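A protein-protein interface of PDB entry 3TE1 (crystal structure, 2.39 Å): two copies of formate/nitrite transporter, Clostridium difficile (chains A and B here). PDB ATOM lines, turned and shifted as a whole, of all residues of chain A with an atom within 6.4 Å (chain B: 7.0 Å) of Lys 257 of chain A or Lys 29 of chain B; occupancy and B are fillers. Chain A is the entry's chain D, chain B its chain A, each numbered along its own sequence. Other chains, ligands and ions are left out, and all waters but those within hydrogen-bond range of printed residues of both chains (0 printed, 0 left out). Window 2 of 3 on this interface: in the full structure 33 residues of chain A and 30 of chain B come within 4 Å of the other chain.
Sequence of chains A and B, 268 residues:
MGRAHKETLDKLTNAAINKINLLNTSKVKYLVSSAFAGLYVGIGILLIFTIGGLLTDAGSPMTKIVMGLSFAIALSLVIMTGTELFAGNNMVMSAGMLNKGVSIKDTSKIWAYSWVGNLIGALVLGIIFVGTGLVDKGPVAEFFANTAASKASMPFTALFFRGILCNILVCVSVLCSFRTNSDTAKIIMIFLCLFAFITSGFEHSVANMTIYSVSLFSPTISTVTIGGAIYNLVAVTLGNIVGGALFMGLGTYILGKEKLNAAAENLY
No position is printed for both chains.
Among the printed residues, pairs that only touch across the chains: Ile 254 of chain A with Lys 29 of chain B (3.0 Å), Leu 255 of chain A with Lys 29 of chain B (3.5 Å), Ile 254 of chain A with Val 32 of chain B (3.7 Å), Leu 255 of chain A with Ser 33 of chain B (3.8 Å) and Leu 255 of chain A with Val 32 of chain B (3.8 Å).
OG of Ser 33 of chain B is in hydrogen-bond range of N of Glu 84 of chain B (2.8 Å).
The side-chain hydroxyl (OG) of Ser 26 of chain B is in hydrogen-bond range of the backbone NH (N) of Lys 29 of chain B.
Printed residues of chain B that touch a printed residue of chain A: Lys 29, Val 32 and Ser 33.
Along chain B the printed residues that touch a printed residue of chain A span positions 29 to 33.
Among the printed residues, 6 pairs touch across the chains.
Among the printed residues, no Asp or Glu carboxylate lies within 4 Å of a Lys or Arg side-chain nitrogen of the other chain.
The side-chain amino group (NZ) of Lys 29 of chain B is in hydrogen-bond range of the backbone carbonyl oxygen (O) of Lys 257 of chain A (2.6 Å).
Of the printed residues of chain B, Ile 254 of chain A touches Lys 29 and Val 32.
Of the printed residues of chain B, Leu 255 of chain A touches Lys 29, Val 32 and Ser 33.
No residue of chain B comes within 4 Å of Gly 256 of chain A.
Printed residues of chain B within 4 Å of Lys 257 of chain A: Lys 29.
Leu 22 of chain B touches none of the printed residues of chain A.
Of the printed residues of chain A, Lys 29 of chain B touches Ile 254, Leu 255 and Lys 257.
The nearest printed residue of chain A that does not touch Val 32 of chain B is Thr 252 of chain A (5.9 Å).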
ATOM      1  N   HIS A   5     -14.700   9.120 -25.112  1.00  0.00           N
ATOM      2  CA  HIS A   5     -14.078   7.855 -24.718  1.00  0.00           C
ATOM      3  C   HIS A   5     -13.723   6.945 -25.902  1.00  0.00           C
ATOM      4  O   HIS A   5     -12.617   6.407 -25.940  1.00  0.00           O
ATOM      5  CB  HIS A   5     -14.958   7.116 -23.709  1.00  0.00           C
ATOM      6  CG  HIS A   5     -15.460   7.978 -22.609  1.00  0.00           C
ATOM      7  ND1 HIS A   5     -14.626   8.672 -21.744  1.00  0.00           N
ATOM      8  CD2 HIS A   5     -16.726   8.268 -22.199  1.00  0.00           C
ATOM      9  CE1 HIS A   5     -15.349   9.348 -20.874  1.00  0.00           C
ATOM     10  NE2 HIS A   5     -16.636   9.109 -21.126  1.00  0.00           N
ATOM     11  N   LYS A   6     -14.626   6.782 -26.879  1.00  0.00           N
ATOM     12  CA  LYS A   6     -14.327   5.924 -28.052  1.00  0.00           C
ATOM     13  C   LYS A   6     -13.062   6.374 -28.763  1.00  0.00           C
ATOM     14  O   LYS A   6     -12.231   5.557 -29.197  1.00  0.00           O
ATOM     15  CB  LYS A   6     -15.470   5.922 -29.084  1.00  0.00           C
ATOM     16  CG  LYS A   6     -16.658   5.052 -28.758  1.00  0.00           C
ATOM     17  CD  LYS A   6     -17.892   5.921 -28.602  1.00  0.00           C
ATOM     18  CE  LYS A   6     -19.163   5.115 -28.776  1.00  0.00           C
ATOM     19  NZ  LYS A   6     -20.375   5.977 -28.667  1.00  0.00           N
ATOM     20  N   LEU A   9     -10.029   5.818 -26.542  1.00  0.00           N
ATOM     21  CA  LEU A   9      -9.600   4.413 -26.660  1.00  0.00           C
ATOM     22  C   LEU A   9      -9.013   4.033 -28.046  1.00  0.00           C
ATOM     23  O   LEU A   9      -8.194   3.116 -28.128  1.00  0.00           O
ATOM     24  CB  LEU A   9     -10.721   3.439 -26.240  1.00  0.00           C
ATOM     25  CG  LEU A   9     -10.514   1.947 -26.553  1.00  0.00           C
ATOM     26  CD1 LEU A   9      -9.342   1.362 -25.756  1.00  0.00           C
ATOM     27  CD2 LEU A   9     -11.792   1.141 -26.316  1.00  0.00           C
ATOM     28  N   LEU A  98      -6.664  -4.989 -24.982  1.00  0.00           N
ATOM     29  CA  LEU A  98      -8.089  -5.193 -24.701  1.00  0.00           C
ATOM     30  C   LEU A  98      -8.984  -4.891 -25.893  1.00  0.00           C
ATOM     31  O   LEU A  98     -10.007  -5.545 -26.107  1.00  0.00           O
ATOM     32  CB  LEU A  98      -8.537  -4.343 -23.512  1.00  0.00           C
ATOM     33  CG  LEU A  98      -8.445  -5.042 -22.155  1.00  0.00           C
ATOM     34  CD1 LEU A  98      -8.283  -4.028 -21.006  1.00  0.00           C
ATOM     35  CD2 LEU A  98      -9.677  -5.912 -21.968  1.00  0.00           C
ATOM     36  N   ASN A  99      -8.613  -3.874 -26.653  1.00  0.00           N
ATOM     37  CA  ASN A  99      -9.379  -3.499 -27.817  1.00  0.00           C
ATOM     38  C   ASN A  99      -8.693  -4.124 -29.029  1.00  0.00           C
ATOM     39  O   ASN A  99      -8.559  -3.504 -30.110  1.00  0.00           O
ATOM     40  CB  ASN A  99      -9.457  -1.979 -27.945  1.00  0.00           C
ATOM     41  CG  ASN A  99     -10.553  -1.534 -28.875  1.00  0.00           C
ATOM     42  OD1 ASN A  99     -11.691  -2.025 -28.819  1.00  0.00           O
ATOM     43  ND2 ASN A  99     -10.212  -0.616 -29.765  1.00  0.00           N
ATOM     44  N   THR A 252     -10.499   2.455 -19.201  1.00  0.00           N
ATOM     45  CA  THR A 252     -10.712   3.298 -20.362  1.00  0.00           C
ATOM     46  C   THR A 252     -11.226   2.403 -21.460  1.00  0.00           C
ATOM     47  O   THR A 252     -11.914   2.878 -22.366  1.00  0.00           O
ATOM     48  CB  THR A 252      -9.420   4.010 -20.789  1.00  0.00           C
ATOM     49  OG1 THR A 252      -8.375   3.042 -20.852  1.00  0.00           O
ATOM     50  CG2 THR A 252      -9.010   5.094 -19.761  1.00  0.00           C
ATOM     51  N   TYR A 253     -10.882   1.107 -21.379  1.00  0.00           N
ATOM     52  CA  TYR A 253     -11.262   0.168 -22.426  1.00  0.00           C
ATOM     53  C   TYR A 253     -12.755  -0.018 -22.416  1.00  0.00           C
ATOM     54  O   TYR A 253     -13.386  -0.130 -23.455  1.00  0.00           O
ATOM     55  CB  TYR A 253     -10.629  -1.210 -22.255  1.00  0.00           C
ATOM     56  CG  TYR A 253     -11.295  -2.201 -23.185  1.00  0.00           C
ATOM     57  CD1 TYR A 253     -11.187  -2.057 -24.579  1.00  0.00           C
ATOM     58  CD2 TYR A 253     -12.056  -3.247 -22.699  1.00  0.00           C
ATOM     59  CE1 TYR A 253     -11.802  -2.954 -25.461  1.00  0.00           C
ATOM     60  CE2 TYR A 253     -12.683  -4.164 -23.586  1.00  0.00           C
ATOM     61  CZ  TYR A 253     -12.551  -4.012 -24.963  1.00  0.00           C
ATOM     62  OH  TYR A 253     -13.157  -4.894 -25.850  1.00  0.00           O
ATOM     63  N   ILE A 254     -13.296  -0.060 -21.211  1.00  0.00           N
ATOM     64  CA  ILE A 254     -14.713  -0.268 -20.973  1.00  0.00           C
ATOM     65  C   ILE A 254     -15.530   0.966 -21.325  1.00  0.00           C
ATOM     66  O   ILE A 254     -16.706   0.861 -21.685  1.00  0.00           O
ATOM     67  CB  ILE A 254     -14.947  -0.641 -19.485  1.00  0.00           C
ATOM     68  CG1 ILE A 254     -14.543  -2.096 -19.220  1.00  0.00           C
ATOM     69  CG2 ILE A 254     -16.385  -0.323 -19.064  1.00  0.00           C
ATOM     70  CD1 ILE A 254     -14.620  -2.511 -17.735  1.00  0.00           C
ATOM     71  N   LEU A 255     -14.902   2.134 -21.231  1.00  0.00           N
ATOM     72  CA  LEU A 255     -15.567   3.400 -21.538  1.00  0.00           C
ATOM     73  C   LEU A 255     -15.632   3.706 -23.050  1.00  0.00           C
ATOM     74  O   LEU A 255     -16.644   4.217 -23.544  1.00  0.00           O
ATOM     75  CB  LEU A 255     -14.882   4.557 -20.788  1.00  0.00           C
ATOM     76  CG  LEU A 255     -14.999   4.664 -19.267  1.00  0.00           C
ATOM     77  CD1 LEU A 255     -14.058   5.721 -18.746  1.00  0.00           C
ATOM     78  CD2 LEU A 255     -16.476   4.882 -18.811  1.00  0.00           C
ATOM     79  N   GLY A 256     -14.577   3.374 -23.790  1.00  0.00           N
ATOM     80  CA  GLY A 256     -14.554   3.651 -25.222  1.00  0.00           C
ATOM     81  C   GLY A 256     -14.882   2.519 -26.185  1.00  0.00           C
ATOM     82  O   GLY A 256     -14.876   2.731 -27.393  1.00  0.00           O
ATOM     83  N   LYS A 257     -15.158   1.313 -25.685  1.00  0.00           N
ATOM     84  CA  LYS A 257     -15.443   0.198 -26.600  1.00  0.00           C
ATOM     85  C   LYS A 257     -16.837   0.280 -27.239  1.00  0.00           C
ATOM     86  O   LYS A 257     -17.845   0.282 -26.526  1.00  0.00           O
ATOM     87  CB  LYS A 257     -15.281  -1.145 -25.885  1.00  0.00           C
ATOM     88  CG  LYS A 257     -15.735  -2.361 -26.687  1.00  0.00           C
ATOM     89  CD  LYS A 257     -15.024  -2.451 -28.032  1.00  0.00           C
ATOM     90  CE  LYS A 257     -15.051  -3.869 -28.524  1.00  0.00           C
ATOM     91  NZ  LYS A 257     -16.336  -4.512 -28.129  1.00  0.00           N
ATOM     92  N   GLU A 258     -16.892   0.324 -28.574  1.00  0.00           N
ATOM     93  CA  GLU A 258     -18.168   0.321 -29.295  1.00  0.00           C
ATOM     94  C   GLU A 258     -18.798  -1.081 -29.355  1.00  0.00           C
ATOM     95  O   GLU A 258     -18.332  -1.946 -30.108  1.00  0.00           O
ATOM     96  CB  GLU A 258     -17.994   0.884 -30.706  1.00  0.00           C
ATOM     97  CG  GLU A 258     -19.310   1.050 -31.471  1.00  0.00           C
ATOM     98  CD  GLU A 258     -19.387   2.360 -32.247  1.00  0.00           C
ATOM     99  OE1 GLU A 258     -18.349   2.787 -32.793  1.00  0.00           O
ATOM    100  OE2 GLU A 258     -20.482   2.962 -32.296  1.00  0.00           O
ATOM    101  N   LYS A 259     -19.866  -1.283 -28.573  1.00  0.00           N
ATOM    102  CA  LYS A 259     -20.546  -2.586 -28.461  1.00  0.00           C
ATOM    103  C   LYS A 259     -22.073  -2.562 -28.690  1.00  0.00           C
ATOM    104  O   LYS A 259     -22.664  -1.537 -29.045  1.00  0.00           O
ATOM    105  CB  LYS A 259     -20.222  -3.257 -27.111  1.00  0.00           C
ATOM    106  CG  LYS A 259     -20.048  -2.280 -25.942  1.00  0.00           C
ATOM    107  CD  LYS A 259     -20.366  -2.925 -24.586  1.00  0.00           C
ATOM    108  CE  LYS A 259     -19.151  -3.595 -23.927  1.00  0.00           C
ATOM    109  NZ  LYS A 259     -18.613  -2.851 -22.720  1.00  0.00           N
ATOM    110  N   LEU B  22     -26.440   7.288 -22.510  1.00  0.00           N
ATOM    111  CA  LEU B  22     -25.344   6.442 -22.055  1.00  0.00           C
ATOM    112  C   LEU B  22     -25.870   5.410 -21.058  1.00  0.00           C
ATOM    113  O   LEU B  22     -25.618   4.208 -21.193  1.00  0.00           O
ATOM    114  CB  LEU B  22     -24.248   7.308 -21.419  1.00  0.00           C
ATOM    115  CG  LEU B  22     -22.922   6.665 -21.046  1.00  0.00           C
ATOM    116  CD1 LEU B  22     -22.330   5.859 -22.196  1.00  0.00           C
ATOM    117  CD2 LEU B  22     -21.950   7.737 -20.571  1.00  0.00           C
ATOM    118  N   LEU B  23     -26.627   5.883 -20.069  1.00  0.00           N
ATOM    119  CA  LEU B  23     -27.165   5.031 -19.005  1.00  0.00           C
ATOM    120  C   LEU B  23     -28.173   3.976 -19.495  1.00  0.00           C
ATOM    121  O   LEU B  23     -28.130   2.819 -19.062  1.00  0.00           O
ATOM    122  CB  LEU B  23     -27.793   5.896 -17.912  1.00  0.00           C
ATOM    123  CG  LEU B  23     -28.688   5.134 -16.942  1.00  0.00           C
ATOM    124  CD1 LEU B  23     -27.921   3.978 -16.323  1.00  0.00           C
ATOM    125  CD2 LEU B  23     -29.231   6.071 -15.873  1.00  0.00           C
ATOM    126  N   THR B  25     -28.187   2.719 -22.307  1.00  0.00           N
ATOM    127  CA  THR B  25     -27.496   1.882 -23.287  1.00  0.00           C
ATOM    128  C   THR B  25     -26.421   1.018 -22.617  1.00  0.00           C
ATOM    129  O   THR B  25     -25.897   0.077 -23.219  1.00  0.00           O
ATOM    130  CB  THR B  25     -26.852   2.735 -24.416  1.00  0.00           C
ATOM    131  OG1 THR B  25     -27.728   3.805 -24.788  1.00  0.00           O
ATOM    132  CG2 THR B  25     -26.569   1.885 -25.638  1.00  0.00           C
ATOM    133  N   SER B  26     -26.105   1.341 -21.365  1.00  0.00           N
ATOM    134  CA  SER B  26     -25.091   0.606 -20.608  1.00  0.00           C
ATOM    135  C   SER B  26     -25.002   1.057 -19.152  1.00  0.00           C
ATOM    136  O   SER B  26     -24.352   2.065 -18.848  1.00  0.00           O
ATOM    137  CB  SER B  26     -23.723   0.744 -21.280  1.00  0.00           C
ATOM    138  OG  SER B  26     -22.732   0.073 -20.532  1.00  0.00           O
ATOM    139  N   LYS B  27     -25.676   0.328 -18.263  1.00  0.00           N
ATOM    140  CA  LYS B  27     -25.579   0.576 -16.825  1.00  0.00           C
ATOM    141  C   LYS B  27     -24.117   0.497 -16.359  1.00  0.00           C
ATOM    142  O   LYS B  27     -23.668   1.311 -15.534  1.00  0.00           O
ATOM    143  CB  LYS B  27     -26.498  -0.387 -16.053  1.00  0.00           C
ATOM    144  CG  LYS B  27     -27.870   0.200 -15.694  1.00  0.00           C
ATOM    145  CD  LYS B  27     -28.886  -0.882 -15.316  1.00  0.00           C
ATOM    146  CE  LYS B  27     -29.770  -1.250 -16.506  1.00  0.00           C
ATOM    147  NZ  LYS B  27     -30.361  -2.614 -16.364  1.00  0.00           N
ATOM    148  N   VAL B  28     -23.382  -0.459 -16.933  1.00  0.00           N
ATOM    149  CA  VAL B  28     -21.964  -0.682 -16.626  1.00  0.00           C
ATOM    150  C   VAL B  28     -21.006   0.413 -17.117  1.00  0.00           C
ATOM    151  O   VAL B  28     -20.110   0.846 -16.368  1.00  0.00           O
ATOM    152  CB  VAL B  28     -21.472  -2.069 -17.162  1.00  0.00           C
ATOM    153  CG1 VAL B  28     -19.952  -2.165 -17.124  1.00  0.00           C
ATOM    154  CG2 VAL B  28     -22.125  -3.204 -16.373  1.00  0.00           C
ATOM    155  N   LYS B  29     -21.155   0.851 -18.371  1.00  0.00           N
ATOM    156  CA  LYS B  29     -20.314   1.955 -18.840  1.00  0.00           C
ATOM    157  C   LYS B  29     -20.538   3.207 -17.972  1.00  0.00           C
ATOM    158  O   LYS B  29     -19.586   3.907 -17.602  1.00  0.00           O
ATOM    159  CB  LYS B  29     -20.545   2.257 -20.320  1.00  0.00           C
ATOM    160  CG  LYS B  29     -19.675   1.445 -21.276  1.00  0.00           C
ATOM    161  CD  LYS B  29     -19.956   1.839 -22.730  1.00  0.00           C
ATOM    162  CE  LYS B  29     -18.891   1.338 -23.697  1.00  0.00           C
ATOM    163  NZ  LYS B  29     -19.082   1.963 -25.041  1.00  0.00           N
ATOM    164  N   TYR B  30     -21.799   3.456 -17.621  1.00  0.00           N
ATOM    165  CA  TYR B  30     -22.149   4.629 -16.833  1.00  0.00           C
ATOM    166  C   TYR B  30     -21.530   4.557 -15.440  1.00  0.00           C
ATOM    167  O   TYR B  30     -20.961   5.545 -14.926  1.00  0.00           O
ATOM    168  CB  TYR B  30     -23.677   4.810 -16.733  1.00  0.00           C
ATOM    169  CG  TYR B  30     -24.026   6.144 -16.120  1.00  0.00           C
ATOM    170  CD1 TYR B  30     -24.106   6.294 -14.737  1.00  0.00           C
ATOM    171  CD2 TYR B  30     -24.208   7.279 -16.922  1.00  0.00           C
ATOM    172  CE1 TYR B  30     -24.386   7.537 -14.159  1.00  0.00           C
ATOM    173  CE2 TYR B  30     -24.475   8.525 -16.356  1.00  0.00           C
ATOM    174  CZ  TYR B  30     -24.565   8.650 -14.975  1.00  0.00           C
ATOM    175  OH  TYR B  30     -24.846   9.875 -14.409  1.00  0.00           O
ATOM    176  N   LEU B  31     -21.645   3.380 -14.829  1.00  0.00           N
ATOM    177  CA  LEU B  31     -21.168   3.192 -13.472  1.00  0.00           C
ATOM    178  C   LEU B  31     -19.635   3.196 -13.418  1.00  0.00           C
ATOM    179  O   LEU B  31     -19.038   3.660 -12.434  1.00  0.00           O
ATOM    180  CB  LEU B  31     -21.783   1.936 -12.845  1.00  0.00           C
ATOM    181  CG  LEU B  31     -23.295   1.971 -12.514  1.00  0.00           C
ATOM    182  CD1 LEU B  31     -23.882   0.531 -12.175  1.00  0.00           C
ATOM    183  CD2 LEU B  31     -23.633   2.969 -11.402  1.00  0.00           C
ATOM    184  N   VAL B  32     -18.987   2.708 -14.475  1.00  0.00           N
ATOM    185  CA  VAL B  32     -17.516   2.746 -14.513  1.00  0.00           C
ATOM    186  C   VAL B  32     -17.043   4.185 -14.480  1.00  0.00           C
ATOM    187  O   VAL B  32     -16.033   4.510 -13.843  1.00  0.00           O
ATOM    188  CB  VAL B  32     -16.928   1.978 -15.735  1.00  0.00           C
ATOM    189  CG1 VAL B  32     -15.487   2.430 -16.054  1.00  0.00           C
ATOM    190  CG2 VAL B  32     -16.964   0.483 -15.476  1.00  0.00           C
ATOM    191  N   SER B  33     -17.799   5.046 -15.158  1.00  0.00           N
ATOM    192  CA  SER B  33     -17.489   6.478 -15.223  1.00  0.00           C
ATOM    193  C   SER B  33     -17.738   7.190 -13.877  1.00  0.00           C
ATOM    194  O   SER B  33     -16.857   7.908 -13.373  1.00  0.00           O
ATOM    195  CB  SER B  33     -18.301   7.128 -16.341  1.00  0.00           C
ATOM    196  OG  SER B  33     -17.885   8.456 -16.582  1.00  0.00           O
ATOM    197  N   SER B  34     -18.922   6.963 -13.303  1.00  0.00           N
ATOM    198  CA  SER B  34     -19.220   7.381 -11.926  1.00  0.00           C
ATOM    199  C   SER B  34     -18.128   7.043 -10.910  1.00  0.00           C
ATOM    200  O   SER B  34     -17.657   7.924 -10.162  1.00  0.00           O
ATOM    201  CB  SER B  34     -20.518   6.754 -11.455  1.00  0.00           C
ATOM    202  OG  SER B  34     -21.514   6.970 -12.429  1.00  0.00           O
ATOM    203  N   GLU B  84     -18.455  10.783 -15.040  1.00  0.00           N
ATOM    204  CA  GLU B  84     -19.731  11.150 -14.395  1.00  0.00           C
ATOM    205  C   GLU B  84     -19.639  11.439 -12.904  1.00  0.00           C
ATOM    206  O   GLU B  84     -19.321  10.539 -12.110  1.00  0.00           O
ATOM    207  CB  GLU B  84     -20.762  10.032 -14.573  1.00  0.00           C
ATOM    208  CG  GLU B  84     -21.405  10.030 -15.917  1.00  0.00           C
ATOM    209  CD  GLU B  84     -22.275  11.257 -16.127  1.00  0.00           C
ATOM    210  OE1 GLU B  84     -23.160  11.532 -15.261  1.00  0.00           O
ATOM    211  OE2 GLU B  84     -22.069  11.935 -17.168  1.00  0.00           O
